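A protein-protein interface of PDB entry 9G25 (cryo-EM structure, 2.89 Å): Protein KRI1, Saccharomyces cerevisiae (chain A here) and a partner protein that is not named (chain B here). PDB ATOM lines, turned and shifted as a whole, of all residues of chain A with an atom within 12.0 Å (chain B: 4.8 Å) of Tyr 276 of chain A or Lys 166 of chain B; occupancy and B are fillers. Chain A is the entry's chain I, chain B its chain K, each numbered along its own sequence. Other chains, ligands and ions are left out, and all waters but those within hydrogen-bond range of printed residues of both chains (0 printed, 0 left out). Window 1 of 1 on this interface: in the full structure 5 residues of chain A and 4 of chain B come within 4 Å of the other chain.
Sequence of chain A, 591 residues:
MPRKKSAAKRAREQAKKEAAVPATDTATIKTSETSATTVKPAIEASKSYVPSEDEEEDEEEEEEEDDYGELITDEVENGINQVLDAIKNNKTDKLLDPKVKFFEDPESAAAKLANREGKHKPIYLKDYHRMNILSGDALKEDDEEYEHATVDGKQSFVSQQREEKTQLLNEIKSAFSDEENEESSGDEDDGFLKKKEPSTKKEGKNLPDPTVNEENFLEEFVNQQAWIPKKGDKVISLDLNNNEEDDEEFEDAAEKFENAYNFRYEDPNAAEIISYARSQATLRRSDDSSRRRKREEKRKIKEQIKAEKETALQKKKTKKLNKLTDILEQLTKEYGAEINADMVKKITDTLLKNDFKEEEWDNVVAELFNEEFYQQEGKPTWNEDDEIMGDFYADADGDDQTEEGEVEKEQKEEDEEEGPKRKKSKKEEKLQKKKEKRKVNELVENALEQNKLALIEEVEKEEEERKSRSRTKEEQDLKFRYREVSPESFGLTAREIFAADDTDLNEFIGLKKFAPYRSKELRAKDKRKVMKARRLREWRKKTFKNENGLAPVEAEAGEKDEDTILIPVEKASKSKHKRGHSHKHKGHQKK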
ATOM      1  N   ARG A 264      -7.888  23.560  10.219  1.00  0.00           N
ATOM      2  CA  ARG A 264      -9.017  23.000  10.952  1.00  0.00           C
ATOM      3  C   ARG A 264      -9.133  23.603  12.346  1.00  0.00           C
ATOM      4  O   ARG A 264     -10.242  23.761  12.869  1.00  0.00           O
ATOM      5  CB  ARG A 264      -8.875  21.477  11.021  1.00  0.00           C
ATOM      6  CG  ARG A 264      -9.957  20.749  11.798  1.00  0.00           C
ATOM      7  CD  ARG A 264     -11.344  21.019  11.252  1.00  0.00           C
ATOM      8  NE  ARG A 264     -12.308  20.057  11.770  1.00  0.00           N
ATOM      9  CZ  ARG A 264     -13.383  20.383  12.472  1.00  0.00           C
ATOM     10  NH1 ARG A 264     -13.680  21.642  12.738  1.00  0.00           N
ATOM     11  NH2 ARG A 264     -14.181  19.418  12.920  1.00  0.00           N
ATOM     12  N   ASP A 267     -11.453  26.549  12.960  1.00  0.00           N
ATOM     13  CA  ASP A 267     -12.845  26.186  13.159  1.00  0.00           C
ATOM     14  C   ASP A 267     -13.047  25.798  14.622  1.00  0.00           C
ATOM     15  O   ASP A 267     -12.323  24.937  15.137  1.00  0.00           O
ATOM     16  CB  ASP A 267     -13.201  25.021  12.227  1.00  0.00           C
ATOM     17  CG  ASP A 267     -14.691  24.690  12.192  1.00  0.00           C
ATOM     18  OD1 ASP A 267     -15.499  25.317  12.899  1.00  0.00           O
ATOM     19  OD2 ASP A 267     -15.056  23.772  11.424  1.00  0.00           O
ATOM     20  N   PRO A 268     -13.991  26.418  15.327  1.00  0.00           N
ATOM     21  CA  PRO A 268     -14.286  25.977  16.692  1.00  0.00           C
ATOM     22  C   PRO A 268     -14.929  24.601  16.710  1.00  0.00           C
ATOM     23  O   PRO A 268     -15.493  24.138  15.714  1.00  0.00           O
ATOM     24  CB  PRO A 268     -15.236  27.057  17.219  1.00  0.00           C
ATOM     25  CG  PRO A 268     -15.857  27.637  16.008  1.00  0.00           C
ATOM     26  CD  PRO A 268     -14.789  27.600  14.952  1.00  0.00           C
ATOM     27  N   ASN A 269     -14.806  23.942  17.864  1.00  0.00           N
ATOM     28  CA  ASN A 269     -15.153  22.544  18.132  1.00  0.00           C
ATOM     29  C   ASN A 269     -14.329  21.604  17.256  1.00  0.00           C
ATOM     30  O   ASN A 269     -14.810  20.528  16.873  1.00  0.00           O
ATOM     31  CB  ASN A 269     -16.652  22.265  17.961  1.00  0.00           C
ATOM     32  CG  ASN A 269     -17.114  21.041  18.731  1.00  0.00           C
ATOM     33  OD1 ASN A 269     -17.609  20.078  18.147  1.00  0.00           O
ATOM     34  ND2 ASN A 269     -16.944  21.069  20.047  1.00  0.00           N
ATOM     35  N   ALA A 270     -13.093  21.979  16.918  1.00  0.00           N
ATOM     36  CA  ALA A 270     -12.218  21.073  16.183  1.00  0.00           C
ATOM     37  C   ALA A 270     -11.530  20.089  17.120  1.00  0.00           C
ATOM     38  O   ALA A 270     -10.950  19.094  16.671  1.00  0.00           O
ATOM     39  CB  ALA A 270     -11.183  21.867  15.392  1.00  0.00           C
ATOM     40  N   GLU A 272     -13.008  18.203  19.304  1.00  0.00           N
ATOM     41  CA  GLU A 272     -13.819  17.001  19.402  1.00  0.00           C
ATOM     42  C   GLU A 272     -13.796  16.227  18.090  1.00  0.00           C
ATOM     43  O   GLU A 272     -14.026  16.787  17.015  1.00  0.00           O
ATOM     44  CB  GLU A 272     -15.256  17.365  19.769  1.00  0.00           C
ATOM     45  CG  GLU A 272     -16.159  16.172  20.007  1.00  0.00           C
ATOM     46  CD  GLU A 272     -17.578  16.578  20.350  1.00  0.00           C
ATOM     47  OE1 GLU A 272     -17.858  17.793  20.378  1.00  0.00           O
ATOM     48  OE2 GLU A 272     -18.413  15.680  20.588  1.00  0.00           O
ATOM     49  N   ILE A 273     -13.512  14.932  18.182  1.00  0.00           N
ATOM     50  CA  ILE A 273     -13.645  14.012  17.059  1.00  0.00           C
ATOM     51  C   ILE A 273     -15.076  13.498  17.065  1.00  0.00           C
ATOM     52  O   ILE A 273     -15.489  12.802  18.000  1.00  0.00           O
ATOM     53  CB  ILE A 273     -12.639  12.854  17.147  1.00  0.00           C
ATOM     54  CG1 ILE A 273     -11.206  13.382  17.142  1.00  0.00           C
ATOM     55  CG2 ILE A 273     -12.840  11.885  15.997  1.00  0.00           C
ATOM     56  CD1 ILE A 273     -10.168  12.300  17.333  1.00  0.00           C
ATOM     57  N   ILE A 274     -15.835  13.839  16.025  1.00  0.00           N
ATOM     58  CA  ILE A 274     -17.255  13.520  16.006  1.00  0.00           C
ATOM     59  C   ILE A 274     -17.442  12.045  15.678  1.00  0.00           C
ATOM     60  O   ILE A 274     -16.828  11.511  14.745  1.00  0.00           O
ATOM     61  CB  ILE A 274     -18.003  14.418  15.003  1.00  0.00           C
ATOM     62  CG1 ILE A 274     -17.889  15.896  15.391  1.00  0.00           C
ATOM     63  CG2 ILE A 274     -19.467  14.051  14.946  1.00  0.00           C
ATOM     64  CD1 ILE A 274     -16.817  16.669  14.646  1.00  0.00           C
ATOM     65  N   SER A 275     -18.274  11.369  16.467  1.00  0.00           N
ATOM     66  CA  SER A 275     -18.661   9.993  16.207  1.00  0.00           C
ATOM     67  C   SER A 275     -20.169   9.933  16.025  1.00  0.00           C
ATOM     68  O   SER A 275     -20.906  10.769  16.554  1.00  0.00           O
ATOM     69  CB  SER A 275     -18.229   9.053  17.338  1.00  0.00           C
ATOM     70  OG  SER A 275     -18.744   9.485  18.584  1.00  0.00           O
ATOM     71  N   TYR A 276     -20.620   8.939  15.269  1.00  0.00           N
ATOM     72  CA  TYR A 276     -22.022   8.811  14.906  1.00  0.00           C
ATOM     73  C   TYR A 276     -22.529   7.428  15.282  1.00  0.00           C
ATOM     74  O   TYR A 276     -21.753   6.477  15.408  1.00  0.00           O
ATOM     75  CB  TYR A 276     -22.242   9.051  13.403  1.00  0.00           C
ATOM     76  CG  TYR A 276     -21.794  10.411  12.916  1.00  0.00           C
ATOM     77  CD1 TYR A 276     -20.481  10.634  12.526  1.00  0.00           C
ATOM     78  CD2 TYR A 276     -22.688  11.470  12.845  1.00  0.00           C
ATOM     79  CE1 TYR A 276     -20.072  11.871  12.082  1.00  0.00           C
ATOM     80  CE2 TYR A 276     -22.286  12.712  12.404  1.00  0.00           C
ATOM     81  CZ  TYR A 276     -20.978  12.906  12.020  1.00  0.00           C
ATOM     82  OH  TYR A 276     -20.570  14.142  11.579  1.00  0.00           O
ATOM     83  N   ALA A 277     -23.844   7.331  15.466  1.00  0.00           N
ATOM     84  CA  ALA A 277     -24.463   6.050  15.771  1.00  0.00           C
ATOM     85  C   ALA A 277     -24.411   5.131  14.558  1.00  0.00           C
ATOM     86  O   ALA A 277     -24.303   5.585  13.417  1.00  0.00           O
ATOM     87  CB  ALA A 277     -25.910   6.255  16.218  1.00  0.00           C
ATOM     88  N   ARG A 278     -24.481   3.822  14.814  1.00  0.00           N
ATOM     89  CA  ARG A 278     -24.349   2.847  13.735  1.00  0.00           C
ATOM     90  C   ARG A 278     -25.578   2.839  12.833  1.00  0.00           C
ATOM     91  O   ARG A 278     -25.481   2.511  11.645  1.00  0.00           O
ATOM     92  CB  ARG A 278     -24.096   1.456  14.317  1.00  0.00           C
ATOM     93  CG  ARG A 278     -22.761   1.321  15.029  1.00  0.00           C
ATOM     94  CD  ARG A 278     -21.623   1.181  14.041  1.00  0.00           C
ATOM     95  NE  ARG A 278     -21.502  -0.172  13.514  1.00  0.00           N
ATOM     96  CZ  ARG A 278     -20.535  -1.018  13.841  1.00  0.00           C
ATOM     97  NH1 ARG A 278     -19.566  -0.673  14.672  1.00  0.00           N
ATOM     98  NH2 ARG A 278     -20.533  -2.238  13.310  1.00  0.00           N
ATOM     99  N   SER A 279     -26.740   3.196  13.373  1.00  0.00           N
ATOM    100  CA  SER A 279     -27.994   3.142  12.632  1.00  0.00           C
ATOM    101  C   SER A 279     -28.496   4.554  12.358  1.00  0.00           C
ATOM    102  O   SER A 279     -28.647   5.355  13.287  1.00  0.00           O
ATOM    103  CB  SER A 279     -29.044   2.346  13.405  1.00  0.00           C
ATOM    104  OG  SER A 279     -29.401   3.010  14.604  1.00  0.00           O
ATOM    105  N   GLN A 280     -28.756   4.853  11.085  1.00  0.00           N
ATOM    106  CA  GLN A 280     -29.367   6.109  10.670  1.00  0.00           C
ATOM    107  C   GLN A 280     -30.536   5.807   9.748  1.00  0.00           C
ATOM    108  O   GLN A 280     -30.479   4.853   8.964  1.00  0.00           O
ATOM    109  CB  GLN A 280     -28.369   7.023   9.946  1.00  0.00           C
ATOM    110  CG  GLN A 280     -27.274   7.605  10.818  1.00  0.00           C
ATOM    111  CD  GLN A 280     -26.009   6.776  10.794  1.00  0.00           C
ATOM    112  OE1 GLN A 280     -25.836   5.911   9.936  1.00  0.00           O
ATOM    113  NE2 GLN A 280     -25.112   7.042  11.734  1.00  0.00           N
ATOM    114  N   ALA A 281     -31.590   6.612   9.841  1.00  0.00           N
ATOM    115  CA  ALA A 281     -32.668   6.528   8.868  1.00  0.00           C
ATOM    116  C   ALA A 281     -32.201   7.113   7.542  1.00  0.00           C
ATOM    117  O   ALA A 281     -31.962   8.318   7.424  1.00  0.00           O
ATOM    118  CB  ALA A 281     -33.906   7.268   9.371  1.00  0.00           C
ATOM    119  N   THR A 282     -32.070   6.251   6.537  1.00  0.00           N
ATOM    120  CA  THR A 282     -31.400   6.621   5.301  1.00  0.00           C
ATOM    121  C   THR A 282     -32.218   6.162   4.105  1.00  0.00           C
ATOM    122  O   THR A 282     -33.112   5.320   4.215  1.00  0.00           O
ATOM    123  CB  THR A 282     -29.989   6.020   5.227  1.00  0.00           C
ATOM    124  OG1 THR A 282     -29.338   6.468   4.032  1.00  0.00           O
ATOM    125  CG2 THR A 282     -30.060   4.503   5.217  1.00  0.00           C
ATOM    126  N   ARG A 284     -30.672   4.785   1.544  1.00  0.00           N
ATOM    127  CA  ARG A 284     -29.868   3.754   0.904  1.00  0.00           C
ATOM    128  C   ARG A 284     -30.496   2.378   1.080  1.00  0.00           C
ATOM    129  O   ARG A 284     -31.001   2.041   2.156  1.00  0.00           O
ATOM    130  CB  ARG A 284     -28.454   3.766   1.484  1.00  0.00           C
ATOM    131  CG  ARG A 284     -27.458   2.900   0.742  1.00  0.00           C
ATOM    132  CD  ARG A 284     -26.068   3.054   1.327  1.00  0.00           C
ATOM    133  NE  ARG A 284     -25.781   4.442   1.666  1.00  0.00           N
ATOM    134  CZ  ARG A 284     -24.583   4.901   2.000  1.00  0.00           C
ATOM    135  NH1 ARG A 284     -23.526   4.106   2.044  1.00  0.00           N
ATOM    136  NH2 ARG A 284     -24.441   6.189   2.294  1.00  0.00           N
ATOM    137  N   THR B 162     -30.161  14.147  20.254  1.00  0.00           N
ATOM    138  CA  THR B 162     -28.751  14.484  20.090  1.00  0.00           C
ATOM    139  C   THR B 162     -28.175  13.880  18.814  1.00  0.00           C
ATOM    140  O   THR B 162     -27.437  14.551  18.084  1.00  0.00           O
ATOM    141  CB  THR B 162     -27.957  14.018  21.309  1.00  0.00           C
ATOM    142  OG1 THR B 162     -28.635  14.426  22.503  1.00  0.00           O
ATOM    143  CG2 THR B 162     -26.563  14.621  21.301  1.00  0.00           C
ATOM    144  N   GLU B 163     -28.523  12.626  18.512  1.00  0.00           N
ATOM    145  CA  GLU B 163     -28.075  12.024  17.254  1.00  0.00           C
ATOM    146  C   GLU B 163     -28.709  12.715  16.048  1.00  0.00           C
ATOM    147  O   GLU B 163     -28.061  12.888  15.002  1.00  0.00           O
ATOM    148  CB  GLU B 163     -28.387  10.529  17.241  1.00  0.00           C
ATOM    149  CG  GLU B 163     -27.746   9.745  18.374  1.00  0.00           C
ATOM    150  CD  GLU B 163     -26.234   9.812  18.349  1.00  0.00           C
ATOM    151  OE1 GLU B 163     -25.636   9.414  17.328  1.00  0.00           O
ATOM    152  OE2 GLU B 163     -25.642  10.261  19.351  1.00  0.00           O
ATOM    153  N   GLU B 164     -29.974  13.128  16.181  1.00  0.00           N
ATOM    154  CA  GLU B 164     -30.640  13.845  15.096  1.00  0.00           C
ATOM    155  C   GLU B 164     -29.939  15.165  14.788  1.00  0.00           C
ATOM    156  O   GLU B 164     -29.702  15.491  13.621  1.00  0.00           O
ATOM    157  CB  GLU B 164     -32.107  14.082  15.449  1.00  0.00           C
ATOM    158  CG  GLU B 164     -33.032  12.954  15.026  1.00  0.00           C
ATOM    159  CD  GLU B 164     -34.493  13.347  15.085  1.00  0.00           C
ATOM    160  OE1 GLU B 164     -35.126  13.131  16.140  1.00  0.00           O
ATOM    161  OE2 GLU B 164     -35.010  13.875  14.077  1.00  0.00           O
ATOM    162  N   GLN B 165     -29.577  15.931  15.822  1.00  0.00           N
ATOM    163  CA  GLN B 165     -28.837  17.169  15.577  1.00  0.00           C
ATOM    164  C   GLN B 165     -27.396  16.899  15.158  1.00  0.00           C
ATOM    165  O   GLN B 165     -26.768  17.747  14.520  1.00  0.00           O
ATOM    166  CB  GLN B 165     -28.870  18.099  16.794  1.00  0.00           C
ATOM    167  CG  GLN B 165     -30.207  18.229  17.494  1.00  0.00           C
ATOM    168  CD  GLN B 165     -31.352  18.491  16.534  1.00  0.00           C
ATOM    169  OE1 GLN B 165     -32.086  17.577  16.156  1.00  0.00           O
ATOM    170  NE2 GLN B 165     -31.509  19.747  16.132  1.00  0.00           N
ATOM    171  N   LYS B 166     -26.849  15.732  15.512  1.00  0.00           N
ATOM    172  CA  LYS B 166     -25.552  15.343  14.963  1.00  0.00           C
ATOM    173  C   LYS B 166     -25.627  15.178  13.453  1.00  0.00           C
ATOM    174  O   LYS B 166     -24.656  15.452  12.741  1.00  0.00           O
ATOM    175  CB  LYS B 166     -25.055  14.045  15.602  1.00  0.00           C
ATOM    176  CG  LYS B 166     -24.396  14.197  16.955  1.00  0.00           C
ATOM    177  CD  LYS B 166     -23.659  12.922  17.327  1.00  0.00           C
ATOM    178  CE  LYS B 166     -23.118  12.984  18.741  1.00  0.00           C
ATOM    179  NZ  LYS B 166     -22.409  11.728  19.111  1.00  0.00           N
ATOM    180  N   LEU B 167     -26.774  14.714  12.953  1.00  0.00           N
ATOM    181  CA  LEU B 167     -26.920  14.544  11.507  1.00  0.00           C
ATOM    182  C   LEU B 167     -26.928  15.871  10.746  1.00  0.00           C
ATOM    183  O   LEU B 167     -26.581  15.895   9.560  1.00  0.00           O
ATOM    184  CB  LEU B 167     -28.187  13.751  11.189  1.00  0.00           C
ATOM    185  CG  LEU B 167     -28.155  12.267  11.551  1.00  0.00           C
ATOM    186  CD1 LEU B 167     -29.418  11.573  11.072  1.00  0.00           C
ATOM    187  CD2 LEU B 167     -26.921  11.603  10.961  1.00  0.00           C
ATOM    188  N   TYR B 168     -27.314  16.982  11.384  1.00  0.00           N
ATOM    189  CA  TYR B 168     -27.446  18.248  10.665  1.00  0.00           C
ATOM    190  C   TYR B 168     -26.611  19.392  11.234  1.00  0.00           C
ATOM    191  O   TYR B 168     -26.748  20.525  10.760  1.00  0.00           O
ATOM    192  CB  TYR B 168     -28.909  18.701  10.605  1.00  0.00           C
ATOM    193  CG  TYR B 168     -29.928  17.596  10.470  1.00  0.00           C
ATOM    194  CD1 TYR B 168     -29.958  16.782   9.345  1.00  0.00           C
ATOM    195  CD2 TYR B 168     -30.889  17.396  11.449  1.00  0.00           C
ATOM    196  CE1 TYR B 168     -30.899  15.776   9.217  1.00  0.00           C
ATOM    197  CE2 TYR B 168     -31.832  16.395  11.330  1.00  0.00           C
ATOM    198  CZ  TYR B 168     -31.834  15.590  10.212  1.00  0.00           C
ATOM    199  OH  TYR B 168     -32.775  14.593  10.090  1.00  0.00           O
ATOM    200  N   LYS B 169     -25.761  19.149  12.230  1.00  0.00           N
ATOM    201  CA  LYS B 169     -24.935  20.212  12.788  1.00  0.00           C
ATOM    202  C   LYS B 169     -23.482  19.767  12.798  1.00  0.00           C
ATOM    203  O   LYS B 169     -23.145  18.651  12.397  1.00  0.00           O
ATOM    204  CB  LYS B 169     -25.371  20.603  14.207  1.00  0.00           C
ATOM    205  CG  LYS B 169     -26.816  21.053  14.338  1.00  0.00           C
ATOM    206  CD  LYS B 169     -27.062  22.371  13.632  1.00  0.00           C
ATOM    207  CE  LYS B 169     -28.472  22.870  13.891  1.00  0.00           C
ATOM    208  NZ  LYS B 169     -29.491  21.998  13.247  1.00  0.00           N
ATOM    209  N   LEU B 171     -19.902  19.232  11.657  1.00  0.00           N
ATOM    210  CA  LEU B 171     -19.280  19.118  10.342  1.00  0.00           C
ATOM    211  C   LEU B 171     -20.330  18.965   9.250  1.00  0.00           C
ATOM    212  O   LEU B 171     -20.066  19.253   8.077  1.00  0.00           O
ATOM    213  CB  LEU B 171     -18.307  17.942  10.322  1.00  0.00           C
ATOM    214  CG  LEU B 171     -16.881  18.239  10.784  1.00  0.00           C
ATOM    215  CD1 LEU B 171     -16.090  16.954  10.929  1.00  0.00           C
ATOM    216  CD2 LEU B 171     -16.199  19.186   9.815  1.00  0.00           C
ATOM    217  N   ASN B 172     -21.524  18.512   9.617  1.00  0.00           N
ATOM    218  CA  ASN B 172     -22.628  18.358   8.683  1.00  0.00           C
ATOM    219  C   ASN B 172     -23.513  19.593   8.611  1.00  0.00           C
ATOM    220  O   ASN B 172     -24.612  19.518   8.054  1.00  0.00           O
ATOM    221  CB  ASN B 172     -23.463  17.134   9.065  1.00  0.00           C
ATOM    222  CG  ASN B 172     -22.798  15.835   8.670  1.00  0.00           C
ATOM    223  OD1 ASN B 172     -21.756  15.833   8.019  1.00  0.00           O
ATOM    224  ND2 ASN B 172     -23.398  14.718   9.063  1.00  0.00           N
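The side-chain carboxylate (OE1) of Glu 163 of chain B is in hydrogen-bond range of the backbone NH (N) of Ala 277 of chain A (3.3 Å).
The side-chain amino group (NZ) of Lys 166 of chain B is in hydrogen-bond range of the backbone carbonyl oxygen (O) of Ser 275 of chain A (3.1 Å).
Leu 171 of chain B touches Arg 264 of chain A (CG to NH2, 3.6 Å).
Leu 171 of chain B touches Ile 274 of chain A.
CE2 of Tyr 276 of chain A touches O of Lys 166 of chain B, 3.6 Å away.
Tyr 276 of chain A touches Asn 172 of chain B (OH to ND2, 3.8 Å).
Of chain B, only Lys 166 (3.6 Å) and Asn 172 (3.8 Å) come within 4 Å of Tyr 276 of chain A.
Of the printed residues of chain A, Lys 166 of chain B touches Ser 275 (3.1 Å) and Tyr 276 (3.6 Å).
No residue of chain A comes within 4 Å of Thr 162 of chain B.
Glu 163 of chain B touches just one residue of chain A: Ala 277 (3.3 Å).
Gln 165 of chain B touches none of the printed residues of chain A.
No residue of chain A comes within 4 Å of Tyr 168 of chain B.
No residue of chain A comes within 4 Å of Lys 169 of chain B.
Leu 171 of chain B touches just these residues of chain A: Arg 264 (3.6 Å) and Ile 274 (3.8 Å).
Asn 172 of chain B touches one residue of chain A.
Printed residues of chain B within 4 Å of Ser 275 of chain A: Lys 166 (3.1 Å).
Of the printed residues of chain B, Ile 274 of chain A touches Leu 171.
Glu 164 of chain B touches none of the printed residues of chain A.
The nearest residue of chain A that does not touch Lys 166 of chain B is Ile 274 of chain A (5.0 Å).
O of Leu 167 of chain B sits close to ND2 of Asn 172 of chain B (3.4 Å).
OD2 of Asp 267 of chain A is in salt-bridge range of NH1 of Arg 264 of chain A (2.9 Å).
NZ of Lys 166 of chain B lies within salt-bridge range of OE2 of Glu 163 of chain B.
Printed residues of chain A that touch a printed residue of chain B: Arg 264, Ile 274, Ser 275, Tyr 276 and Ala 277.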
